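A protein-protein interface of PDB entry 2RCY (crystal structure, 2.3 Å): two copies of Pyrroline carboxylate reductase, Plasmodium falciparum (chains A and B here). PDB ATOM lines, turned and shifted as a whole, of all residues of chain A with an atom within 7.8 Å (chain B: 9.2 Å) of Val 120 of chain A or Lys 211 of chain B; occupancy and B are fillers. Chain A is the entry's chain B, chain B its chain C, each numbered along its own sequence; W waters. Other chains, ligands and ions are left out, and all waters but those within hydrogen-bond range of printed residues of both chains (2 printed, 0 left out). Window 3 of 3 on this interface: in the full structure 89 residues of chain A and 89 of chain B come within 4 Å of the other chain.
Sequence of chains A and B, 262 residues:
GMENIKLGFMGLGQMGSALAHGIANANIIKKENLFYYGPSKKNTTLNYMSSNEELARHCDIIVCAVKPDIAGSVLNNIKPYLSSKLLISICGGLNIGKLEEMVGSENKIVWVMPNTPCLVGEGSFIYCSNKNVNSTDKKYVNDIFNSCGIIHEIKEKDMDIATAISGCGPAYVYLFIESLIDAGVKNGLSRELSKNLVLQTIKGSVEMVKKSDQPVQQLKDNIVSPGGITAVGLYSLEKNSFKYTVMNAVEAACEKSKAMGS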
ATOM      1  N   ALA A  18      -5.445   9.691   5.415  1.00  0.00           N
ATOM      2  CA  ALA A  18      -6.169  10.940   5.164  1.00  0.00           C
ATOM      3  C   ALA A  18      -6.963  11.390   6.389  1.00  0.00           C
ATOM      4  O   ALA A  18      -6.995  12.580   6.708  1.00  0.00           O
ATOM      5  CB  ALA A  18      -7.085  10.795   3.952  1.00  0.00           C
ATOM      6  N   HIS A  21      -4.208  12.102   9.449  1.00  0.00           N
ATOM      7  CA  HIS A  21      -3.470  13.357   9.281  1.00  0.00           C
ATOM      8  C   HIS A  21      -4.382  14.583   9.321  1.00  0.00           C
ATOM      9  O   HIS A  21      -3.934  15.680   9.656  1.00  0.00           O
ATOM     10  CB  HIS A  21      -2.636  13.342   7.995  1.00  0.00           C
ATOM     11  CG  HIS A  21      -1.600  12.260   7.959  1.00  0.00           C
ATOM     12  ND1 HIS A  21      -1.583  11.278   6.993  1.00  0.00           N
ATOM     13  CD2 HIS A  21      -0.554  12.001   8.779  1.00  0.00           C
ATOM     14  CE1 HIS A  21      -0.566  10.464   7.214  1.00  0.00           C
ATOM     15  NE2 HIS A  21       0.074  10.879   8.292  1.00  0.00           N
ATOM     16  N   GLY A  22      -5.653  14.388   8.979  1.00  0.00           N
ATOM     17  CA  GLY A  22      -6.658  15.446   9.072  1.00  0.00           C
ATOM     18  C   GLY A  22      -6.986  15.790  10.513  1.00  0.00           C
ATOM     19  O   GLY A  22      -7.213  16.954  10.849  1.00  0.00           O
ATOM     20  N   ASN A  25      -3.598  17.475  12.034  1.00  0.00           N
ATOM     21  CA  ASN A  25      -3.425  18.875  11.636  1.00  0.00           C
ATOM     22  C   ASN A  25      -4.411  19.827  12.314  1.00  0.00           C
ATOM     23  O   ASN A  25      -4.156  21.030  12.413  1.00  0.00           O
ATOM     24  CB  ASN A  25      -3.518  19.022  10.114  1.00  0.00           C
ATOM     25  CG  ASN A  25      -2.350  18.375   9.388  1.00  0.00           C
ATOM     26  OD1 ASN A  25      -1.250  18.253   9.929  1.00  0.00           O
ATOM     27  ND2 ASN A  25      -2.588  17.958   8.149  1.00  0.00           N
ATOM     28  N   ASN A 115     -14.669  10.849   3.772  1.00  0.00           N
ATOM     29  CA  ASN A 115     -14.045  10.965   2.453  1.00  0.00           C
ATOM     30  C   ASN A 115     -12.644  11.577   2.533  1.00  0.00           C
ATOM     31  O   ASN A 115     -12.293  12.198   3.537  1.00  0.00           O
ATOM     32  CB  ASN A 115     -14.953  11.689   1.445  1.00  0.00           C
ATOM     33  CG  ASN A 115     -15.334  13.094   1.879  1.00  0.00           C
ATOM     34  OD1 ASN A 115     -14.755  13.659   2.805  1.00  0.00           O
ATOM     35  ND2 ASN A 115     -16.314  13.669   1.193  1.00  0.00           N
ATOM     36  N   THR A 116     -11.846  11.382   1.482  1.00  0.00           N
ATOM     37  CA  THR A 116     -10.437  11.818   1.464  1.00  0.00           C
ATOM     38  C   THR A 116     -10.182  13.321   1.683  1.00  0.00           C
ATOM     39  O   THR A 116      -9.159  13.679   2.267  1.00  0.00           O
ATOM     40  CB  THR A 116      -9.678  11.340   0.195  1.00  0.00           C
ATOM     41  OG1 THR A 116     -10.415  11.691  -0.983  1.00  0.00           O
ATOM     42  CG2 THR A 116      -9.465   9.835   0.227  1.00  0.00           C
ATOM     43  N   PRO A 117     -11.090  14.204   1.206  1.00  0.00           N
ATOM     44  CA  PRO A 117     -10.963  15.639   1.484  1.00  0.00           C
ATOM     45  C   PRO A 117     -10.802  16.040   2.956  1.00  0.00           C
ATOM     46  O   PRO A 117     -10.583  17.217   3.241  1.00  0.00           O
ATOM     47  CB  PRO A 117     -12.274  16.206   0.941  1.00  0.00           C
ATOM     48  CG  PRO A 117     -12.629  15.303  -0.156  1.00  0.00           C
ATOM     49  CD  PRO A 117     -12.249  13.943   0.329  1.00  0.00           C
ATOM     50  N   CYS A 118     -10.907  15.082   3.876  1.00  0.00           N
ATOM     51  CA  CYS A 118     -10.650  15.347   5.291  1.00  0.00           C
ATOM     52  C   CYS A 118      -9.163  15.589   5.556  1.00  0.00           C
ATOM     53  O   CYS A 118      -8.798  16.180   6.574  1.00  0.00           O
ATOM     54  CB  CYS A 118     -11.186  14.214   6.172  1.00  0.00           C
ATOM     55  SG  CYS A 118     -10.298  12.644   6.038  1.00  0.00           S
ATOM     56  N   LEU A 119      -8.318  15.133   4.630  1.00  0.00           N
ATOM     57  CA  LEU A 119      -6.873  15.369   4.681  1.00  0.00           C
ATOM     58  C   LEU A 119      -6.552  16.864   4.662  1.00  0.00           C
ATOM     59  O   LEU A 119      -5.653  17.318   5.371  1.00  0.00           O
ATOM     60  CB  LEU A 119      -6.171  14.655   3.517  1.00  0.00           C
ATOM     61  CG  LEU A 119      -4.650  14.786   3.357  1.00  0.00           C
ATOM     62  CD1 LEU A 119      -3.901  13.997   4.426  1.00  0.00           C
ATOM     63  CD2 LEU A 119      -4.216  14.337   1.970  1.00  0.00           C
ATOM     64  N   VAL A 120      -7.292  17.619   3.852  1.00  0.00           N
ATOM     65  CA  VAL A 120      -7.170  19.080   3.823  1.00  0.00           C
ATOM     66  C   VAL A 120      -8.194  19.758   4.747  1.00  0.00           C
ATOM     67  O   VAL A 120      -8.488  20.948   4.602  1.00  0.00           O
ATOM     68  CB  VAL A 120      -7.252  19.656   2.375  1.00  0.00           C
ATOM     69  CG1 VAL A 120      -5.997  19.308   1.587  1.00  0.00           C
ATOM     70  CG2 VAL A 120      -8.505  19.171   1.646  1.00  0.00           C
ATOM     71  N   GLY A 121      -8.720  18.988   5.699  1.00  0.00           N
ATOM     72  CA  GLY A 121      -9.663  19.491   6.698  1.00  0.00           C
ATOM     73  C   GLY A 121     -11.009  19.907   6.135  1.00  0.00           C
ATOM     74  O   GLY A 121     -11.682  20.774   6.698  1.00  0.00           O
ATOM     75  N   GLU A 122     -11.404  19.284   5.027  1.00  0.00           N
ATOM     76  CA  GLU A 122     -12.651  19.625   4.346  1.00  0.00           C
ATOM     77  C   GLU A 122     -13.461  18.373   3.999  1.00  0.00           C
ATOM     78  O   GLU A 122     -14.053  18.274   2.923  1.00  0.00           O
ATOM     79  CB  GLU A 122     -12.357  20.459   3.094  1.00  0.00           C
ATOM     80  CG  GLU A 122     -13.445  21.470   2.750  1.00  0.00           C
ATOM     81  CD  GLU A 122     -13.587  22.561   3.796  1.00  0.00           C
ATOM     82  OE1 GLU A 122     -12.555  23.135   4.206  1.00  0.00           O
ATOM     83  OE2 GLU A 122     -14.733  22.845   4.203  1.00  0.00           O
ATOM     84  N   GLY A 123     -13.488  17.423   4.930  1.00  0.00           N
ATOM     85  CA  GLY A 123     -14.183  16.158   4.728  1.00  0.00           C
ATOM     86  C   GLY A 123     -15.688  16.237   4.892  1.00  0.00           C
ATOM     87  O   GLY A 123     -16.213  17.153   5.526  1.00  0.00           O
ATOM     88  N   SER A 147     -13.734  18.750  13.277  1.00  0.00           N
ATOM     89  CA  SER A 147     -12.434  19.420  13.298  1.00  0.00           C
ATOM     90  C   SER A 147     -11.749  19.401  11.930  1.00  0.00           C
ATOM     91  O   SER A 147     -10.926  20.269  11.630  1.00  0.00           O
ATOM     92  CB  SER A 147     -11.521  18.794  14.358  1.00  0.00           C
ATOM     93  OG  SER A 147     -11.077  17.508  13.962  1.00  0.00           O
ATOM     94  N   CYS A 148     -12.091  18.408  11.112  1.00  0.00           N
ATOM     95  CA  CYS A 148     -11.542  18.286   9.763  1.00  0.00           C
ATOM     96  C   CYS A 148     -12.633  18.110   8.701  1.00  0.00           C
ATOM     97  O   CYS A 148     -12.428  17.442   7.684  1.00  0.00           O
ATOM     98  CB  CYS A 148     -10.525  17.141   9.700  1.00  0.00           C
ATOM     99  SG  CYS A 148     -11.200  15.505  10.062  1.00  0.00           S
ATOM    100  N   GLY A 149     -13.791  18.723   8.942  1.00  0.00           N
ATOM    101  CA  GLY A 149     -14.907  18.668   8.003  1.00  0.00           C
ATOM    102  C   GLY A 149     -16.259  18.875   8.657  1.00  0.00           C
ATOM    103  O   GLY A 149     -16.358  19.510   9.707  1.00  0.00           O
ATOM    104  N   TYR A 174     -13.744  14.618  -9.071  1.00  0.00           N
ATOM    105  CA  TYR A 174     -12.411  14.578  -9.678  1.00  0.00           C
ATOM    106  C   TYR A 174     -12.495  14.296 -11.176  1.00  0.00           C
ATOM    107  O   TYR A 174     -11.767  14.900 -11.963  1.00  0.00           O
ATOM    108  CB  TYR A 174     -11.514  13.520  -9.023  1.00  0.00           C
ATOM    109  CG  TYR A 174     -11.106  13.786  -7.588  1.00  0.00           C
ATOM    110  CD1 TYR A 174     -10.763  15.068  -7.152  1.00  0.00           C
ATOM    111  CD2 TYR A 174     -11.027  12.737  -6.671  1.00  0.00           C
ATOM    112  CE1 TYR A 174     -10.381  15.296  -5.831  1.00  0.00           C
ATOM    113  CE2 TYR A 174     -10.645  12.954  -5.358  1.00  0.00           C
ATOM    114  CZ  TYR A 174     -10.322  14.231  -4.944  1.00  0.00           C
ATOM    115  OH  TYR A 174      -9.944  14.433  -3.639  1.00  0.00           O
ATOM    116  N   LYS A 195      -7.074  24.095 -15.335  1.00  0.00           N
ATOM    117  CA  LYS A 195      -7.259  23.727 -13.930  1.00  0.00           C
ATOM    118  C   LYS A 195      -7.706  24.918 -13.082  1.00  0.00           C
ATOM    119  O   LYS A 195      -8.691  24.823 -12.351  1.00  0.00           O
ATOM    120  CB  LYS A 195      -5.979  23.103 -13.360  1.00  0.00           C
ATOM    121  CG  LYS A 195      -6.125  22.526 -11.948  1.00  0.00           C
ATOM    122  CD  LYS A 195      -4.915  21.686 -11.543  1.00  0.00           C
ATOM    123  CE  LYS A 195      -3.735  22.549 -11.106  1.00  0.00           C
ATOM    124  NZ  LYS A 195      -2.546  21.721 -10.749  1.00  0.00           N
ATOM    125  N   LEU A 199     -11.447  25.007 -11.356  1.00  0.00           N
ATOM    126  CA  LEU A 199     -11.556  25.006  -9.897  1.00  0.00           C
ATOM    127  C   LEU A 199     -12.277  26.242  -9.362  1.00  0.00           C
ATOM    128  O   LEU A 199     -13.127  26.126  -8.479  1.00  0.00           O
ATOM    129  CB  LEU A 199     -10.180  24.838  -9.241  1.00  0.00           C
ATOM    130  CG  LEU A 199      -9.469  23.488  -9.420  1.00  0.00           C
ATOM    131  CD1 LEU A 199      -8.110  23.499  -8.732  1.00  0.00           C
ATOM    132  CD2 LEU A 199     -10.315  22.315  -8.921  1.00  0.00           C
ATOM    133  N   GLN B 200     -20.577  19.900   0.218  1.00  0.00           N
ATOM    134  CA  GLN B 200     -19.394  19.656   1.044  1.00  0.00           C
ATOM    135  C   GLN B 200     -18.424  18.682   0.376  1.00  0.00           C
ATOM    136  O   GLN B 200     -17.204  18.824   0.500  1.00  0.00           O
ATOM    137  CB  GLN B 200     -19.802  19.167   2.443  1.00  0.00           C
ATOM    138  CG  GLN B 200     -18.647  18.843   3.405  1.00  0.00           C
ATOM    139  CD  GLN B 200     -17.708  20.016   3.676  1.00  0.00           C
ATOM    140  OE1 GLN B 200     -18.024  21.172   3.389  1.00  0.00           O
ATOM    141  NE2 GLN B 200     -16.544  19.713   4.238  1.00  0.00           N
ATOM    142  N   THR B 201     -18.976  17.699  -0.332  1.00  0.00           N
ATOM    143  CA  THR B 201     -18.178  16.735  -1.090  1.00  0.00           C
ATOM    144  C   THR B 201     -17.403  17.426  -2.214  1.00  0.00           C
ATOM    145  O   THR B 201     -16.219  17.150  -2.424  1.00  0.00           O
ATOM    146  CB  THR B 201     -19.060  15.611  -1.669  1.00  0.00           C
ATOM    147  OG1 THR B 201     -19.711  14.920  -0.599  1.00  0.00           O
ATOM    148  CG2 THR B 201     -18.230  14.623  -2.452  1.00  0.00           C
ATOM    149  N   ILE B 202     -18.079  18.329  -2.919  1.00  0.00           N
ATOM    150  CA  ILE B 202     -17.461  19.091  -4.000  1.00  0.00           C
ATOM    151  C   ILE B 202     -16.426  20.083  -3.462  1.00  0.00           C
ATOM    152  O   ILE B 202     -15.325  20.185  -4.004  1.00  0.00           O
ATOM    153  CB  ILE B 202     -18.515  19.823  -4.865  1.00  0.00           C
ATOM    154  CG1 ILE B 202     -19.509  18.821  -5.459  1.00  0.00           C
ATOM    155  CG2 ILE B 202     -17.836  20.604  -5.979  1.00  0.00           C
ATOM    156  CD1 ILE B 202     -20.722  19.452  -6.107  1.00  0.00           C
ATOM    157  N   LYS B 203     -16.784  20.794  -2.393  1.00  0.00           N
ATOM    158  CA  LYS B 203     -15.892  21.766  -1.755  1.00  0.00           C
ATOM    159  C   LYS B 203     -14.567  21.131  -1.340  1.00  0.00           C
ATOM    160  O   LYS B 203     -13.499  21.706  -1.564  1.00  0.00           O
ATOM    161  CB  LYS B 203     -16.572  22.406  -0.541  1.00  0.00           C
ATOM    162  CG  LYS B 203     -15.839  23.609   0.041  1.00  0.00           C
ATOM    163  CD  LYS B 203     -16.511  24.092   1.321  1.00  0.00           C
ATOM    164  CE  LYS B 203     -15.960  25.436   1.778  1.00  0.00           C
ATOM    165  NZ  LYS B 203     -14.522  25.361   2.167  1.00  0.00           N
ATOM    166  N   GLY B 204     -14.650  19.944  -0.742  1.00  0.00           N
ATOM    167  CA  GLY B 204     -13.472  19.205  -0.309  1.00  0.00           C
ATOM    168  C   GLY B 204     -12.640  18.665  -1.456  1.00  0.00           C
ATOM    169  O   GLY B 204     -11.409  18.661  -1.384  1.00  0.00           O
ATOM    170  N   SER B 205     -13.313  18.203  -2.509  1.00  0.00           N
ATOM    171  CA  SER B 205     -12.642  17.667  -3.695  1.00  0.00           C
ATOM    172  C   SER B 205     -11.843  18.736  -4.439  1.00  0.00           C
ATOM    173  O   SER B 205     -10.721  18.483  -4.882  1.00  0.00           O
ATOM    174  CB  SER B 205     -13.652  17.016  -4.640  1.00  0.00           C
ATOM    175  OG  SER B 205     -14.357  15.973  -3.994  1.00  0.00           O
ATOM    176  N   VAL B 206     -12.431  19.924  -4.574  1.00  0.00           N
ATOM    177  CA  VAL B 206     -11.763  21.071  -5.192  1.00  0.00           C
ATOM    178  C   VAL B 206     -10.509  21.447  -4.402  1.00  0.00           C
ATOM    179  O   VAL B 206      -9.463  21.736  -4.986  1.00  0.00           O
ATOM    180  CB  VAL B 206     -12.724  22.287  -5.317  1.00  0.00           C
ATOM    181  CG1 VAL B 206     -11.969  23.564  -5.684  1.00  0.00           C
ATOM    182  CG2 VAL B 206     -13.808  22.001  -6.342  1.00  0.00           C
ATOM    183  N   GLU B 207     -10.627  21.415  -3.075  1.00  0.00           N
ATOM    184  CA  GLU B 207      -9.529  21.733  -2.169  1.00  0.00           C
ATOM    185  C   GLU B 207      -8.383  20.721  -2.267  1.00  0.00           C
ATOM    186  O   GLU B 207      -7.217  21.083  -2.114  1.00  0.00           O
ATOM    187  CB  GLU B 207     -10.045  21.814  -0.728  1.00  0.00           C
ATOM    188  CG  GLU B 207      -9.246  22.738   0.180  1.00  0.00           C
ATOM    189  CD  GLU B 207      -9.507  24.207  -0.104  1.00  0.00           C
ATOM    190  OE1 GLU B 207     -10.617  24.691   0.217  1.00  0.00           O
ATOM    191  OE2 GLU B 207      -8.597  24.876  -0.641  1.00  0.00           O
ATOM    192  N   MET B 208      -8.722  19.458  -2.523  1.00  0.00           N
ATOM    193  CA  MET B 208      -7.722  18.397  -2.679  1.00  0.00           C
ATOM    194  C   MET B 208      -6.912  18.571  -3.960  1.00  0.00           C
ATOM    195  O   MET B 208      -5.692  18.395  -3.957  1.00  0.00           O
ATOM    196  CB  MET B 208      -8.384  17.017  -2.657  1.00  0.00           C
ATOM    197  CG  MET B 208      -8.858  16.570  -1.286  1.00  0.00           C
ATOM    198  SD  MET B 208      -7.419  15.956  -0.124  1.00  0.00           S
ATOM    199  CE  MET B 208      -7.085  14.213  -0.925  1.00  0.00           C
ATOM    200  N   VAL B 209      -7.598  18.917  -5.047  1.00  0.00           N
ATOM    201  CA  VAL B 209      -6.949  19.223  -6.323  1.00  0.00           C
ATOM    202  C   VAL B 209      -6.059  20.464  -6.178  1.00  0.00           C
ATOM    203  O   VAL B 209      -4.974  20.539  -6.762  1.00  0.00           O
ATOM    204  CB  VAL B 209      -7.994  19.445  -7.449  1.00  0.00           C
ATOM    205  CG1 VAL B 209      -7.314  19.807  -8.764  1.00  0.00           C
ATOM    206  CG2 VAL B 209      -8.859  18.208  -7.629  1.00  0.00           C
ATOM    207  N   LYS B 210      -6.538  21.420  -5.382  1.00  0.00           N
ATOM    208  CA  LYS B 210      -5.855  22.684  -5.129  1.00  0.00           C
ATOM    209  C   LYS B 210      -4.522  22.499  -4.402  1.00  0.00           C
ATOM    210  O   LYS B 210      -3.524  23.128  -4.757  1.00  0.00           O
ATOM    211  CB  LYS B 210      -6.758  23.580  -4.278  1.00  0.00           C
ATOM    212  CG  LYS B 210      -6.684  25.060  -4.581  1.00  0.00           C
ATOM    213  CD  LYS B 210      -7.945  25.519  -5.284  1.00  0.00           C
ATOM    214  CE  LYS B 210      -8.171  27.006  -5.092  1.00  0.00           C
ATOM    215  NZ  LYS B 210      -9.531  27.421  -5.545  1.00  0.00           N
ATOM    216  N   LYS B 211      -4.513  21.624  -3.396  1.00  0.00           N
ATOM    217  CA  LYS B 211      -3.415  21.556  -2.428  1.00  0.00           C
ATOM    218  C   LYS B 211      -2.482  20.349  -2.568  1.00  0.00           C
ATOM    219  O   LYS B 211      -1.378  20.352  -2.015  1.00  0.00           O
ATOM    220  CB  LYS B 211      -3.973  21.620  -0.999  1.00  0.00           C
ATOM    221  CG  LYS B 211      -4.703  22.916  -0.668  1.00  0.00           C
ATOM    222  CD  LYS B 211      -5.178  22.927   0.775  1.00  0.00           C
ATOM    223  CE  LYS B 211      -5.798  24.266   1.142  1.00  0.00           C
ATOM    224  NZ  LYS B 211      -6.258  24.293   2.558  1.00  0.00           N
ATOM    225  N   SER B 212      -2.917  19.328  -3.300  1.00  0.00           N
ATOM    226  CA  SER B 212      -2.141  18.094  -3.422  1.00  0.00           C
ATOM    227  C   SER B 212      -1.103  18.141  -4.542  1.00  0.00           C
ATOM    228  O   SER B 212      -1.294  18.820  -5.555  1.00  0.00           O
ATOM    229  CB  SER B 212      -3.068  16.889  -3.617  1.00  0.00           C
ATOM    230  OG  SER B 212      -2.325  15.691  -3.767  1.00  0.00           O
ATOM    231  N   ASP B 213      -0.005  17.415  -4.336  1.00  0.00           N
ATOM    232  CA  ASP B 213       1.044  17.256  -5.342  1.00  0.00           C
ATOM    233  C   ASP B 213       0.678  16.178  -6.364  1.00  0.00           C
ATOM    234  O   ASP B 213       1.277  16.098  -7.439  1.00  0.00           O
ATOM    235  CB  ASP B 213       2.393  16.936  -4.677  1.00  0.00           C
ATOM    236  CG  ASP B 213       2.310  15.776  -3.689  1.00  0.00           C
ATOM    237  OD1 ASP B 213       1.503  15.844  -2.736  1.00  0.00           O
ATOM    238  OD2 ASP B 213       3.072  14.799  -3.857  1.00  0.00           O
ATOM    239  N   GLN B 214      -0.311  15.357  -6.014  1.00  0.00           N
ATOM    240  CA  GLN B 214      -0.815  14.300  -6.891  1.00  0.00           C
ATOM    241  C   GLN B 214      -1.811  14.884  -7.894  1.00  0.00           C
ATOM    242  O   GLN B 214      -2.623  15.739  -7.526  1.00  0.00           O
ATOM    243  CB  GLN B 214      -1.508  13.208  -6.069  1.00  0.00           C
ATOM    244  CG  GLN B 214      -0.633  12.532  -5.021  1.00  0.00           C
ATOM    245  CD  GLN B 214      -1.397  11.524  -4.170  1.00  0.00           C
ATOM    246  OE1 GLN B 214      -2.595  11.675  -3.923  1.00  0.00           O
ATOM    247  NE2 GLN B 214      -0.699  10.492  -3.714  1.00  0.00           N
ATOM    248  N   PRO B 215      -1.759  14.426  -9.162  1.00  0.00           N
ATOM    249  CA  PRO B 215      -2.732  14.858 -10.175  1.00  0.00           C
ATOM    250  C   PRO B 215      -4.166  14.431  -9.841  1.00  0.00           C
ATOM    251  O   PRO B 215      -4.369  13.561  -8.989  1.00  0.00           O
ATOM    252  CB  PRO B 215      -2.249  14.154 -11.449  1.00  0.00           C
ATOM    253  CG  PRO B 215      -1.440  12.999 -10.969  1.00  0.00           C
ATOM    254  CD  PRO B 215      -0.772  13.485  -9.723  1.00  0.00           C
ATOM    255  N   LEU B 219      -5.716  11.271  -7.343  1.00  0.00           N
ATOM    256  CA  LEU B 219      -6.637  11.557  -6.245  1.00  0.00           C
ATOM    257  C   LEU B 219      -7.932  10.765  -6.414  1.00  0.00           C
ATOM    258  O   LEU B 219      -8.533  10.326  -5.430  1.00  0.00           O
ATOM    259  CB  LEU B 219      -6.943  13.057  -6.174  1.00  0.00           C
ATOM    260  CG  LEU B 219      -5.796  14.023  -5.851  1.00  0.00           C
ATOM    261  CD1 LEU B 219      -6.162  15.442  -6.260  1.00  0.00           C
ATOM    262  CD2 LEU B 219      -5.417  13.968  -4.375  1.00  0.00           C
HETATM  263  O   HOH W   1     -15.585  16.758   1.188  1.00  0.00           O
HETATM  264  O   HOH W   2      -8.468  11.834  -3.010  1.00  0.00           O
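The side-chain carboxylate (OE2) of Glu 122 of chain A is in salt-bridge range of the side-chain amino group (NZ) of Lys 203 of chain B. O of Gly 123 of chain A sits at hydrogen-bond distance from NE2 of Gln 200 of chain B (2.9 Å). O of Glu 122 of chain A sits at hydrogen-bond distance from NE2 of Gln 200 of chain B (3.2 Å). O of Thr 116 of chain A lies close to SD of Met 208 of chain B, at 3.7 Å.
The backbone carbonyl oxygen (O) of Cys 148 of chain A is in hydrogen-bond range of the backbone NH (N) of Gly 123 of chain A (3.0 Å). The backbone carbonyl oxygen of Pro 117 of chain A lies within hydrogen-bond range of the backbone NH of Gly 123 of chain A, 3.4 Å away. O of Cys 148 of chain A is in hydrogen-bond range of N of Glu 122 of chain A, 3.4 Å away. N of Glu 122 of chain A lies within hydrogen-bond range of O of Pro 117 of chain A. The side-chain hydroxyl (OG) of Ser 205 of chain B sits at hydrogen-bond distance from the backbone carbonyl oxygen (O) of Thr 201 of chain B (2.7 Å).
CG of Pro 117 of chain A touches N of Ser 205 of chain B, at 3.8 Å. Glu 207 of chain B touches Val 120 of chain A (CB to CG2, 3.9 Å). CG1 of Val 120 of chain A touches CD of Lys 211 of chain B, at 3.8 Å. O of Glu 122 of chain A touches CA of Gly 204 of chain B, at 3.4 Å. Tyr 174 of chain A touches Ser 205 of chain B. Tyr 174 of chain A touches Met 208 of chain B (OH to CB, 3.2 Å). CD1 of Tyr 174 of chain A touches CG2 of Val 209 of chain B, at 3.7 Å. Tyr 174 of chain A touches Leu 219 of chain B (CE2 to O, 3.4 Å). Leu 199 of chain A touches Val 206 of chain B (CD2 to CG1, 3.8 Å). CG1 of Val 209 of chain B touches CD1 of Leu 199 of chain A, at 3.8 Å.
Val 120 of chain A touches just these residues of chain B: Glu 207, Met 208 and Lys 211. Of the printed residues of chain A, Lys 211 of chain B touches Val 120. Leu 119 of chain A touches none of the printed residues of chain B. No residue of chain B comes within 4 Å of Gly 121 of chain A. Printed residues of chain B within 4 Å of Thr 116 of chain A: Met 208 (3.7 Å). Of the printed residues of chain B, Leu 199 of chain A touches Val 206 (3.8 Å), Val 209 (3.8 Å) and Lys 210 (3.9995 Å). Printed residues of chain A within 4 Å of Gly 204 of chain B: Pro 117 (3.5 Å) and Glu 122 (3.4 Å). Of the printed residues of chain A, Val 206 of chain B touches Leu 199 (3.8 Å). Pro 215 of chain B touches none of the printed residues of chain A. Ala 18 of chain A touches none of the printed residues of chain B. The nearest printed residue of chain A that does not touch Lys 211 of chain B is Glu 122 of chain A (6.6 Å). The nearest printed residue of chain B that does not touch Tyr 174 of chain A is Gly 204 of chain B (5.0 Å).
Hydrophobic or aromatic side chains of chain A that line the printed part of chain B: Pro 117, Val 120, Tyr 174 and Leu 199. Of the 17 printed residues of chain B, 11 touch a printed residue of chain A. Hydrophobic or aromatic side chains of chain B that line the printed part of chain A: Val 206, Met 208, Val 209 and Leu 219. Among the printed residues, 18 pairs touch across the chains.
No position is printed for both chains. Of the 18 pairs that touch across the chains among the printed residues, none has its exchanged pair printed and touching as well.
Water W1 lies within hydrogen-bond range of O of Gln 200 of chain B (2.7 Å), O of Glu 122 of chain A (2.8 Å) and ND2 of Asn 115 of chain A (3.2 Å). Water W2 lies within hydrogen-bond range of OG1 of Thr 116 of chain A (2.8 Å), O of Leu 219 of chain B (2.9 Å) and OH of Tyr 174 of chain A (3.1 Å).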
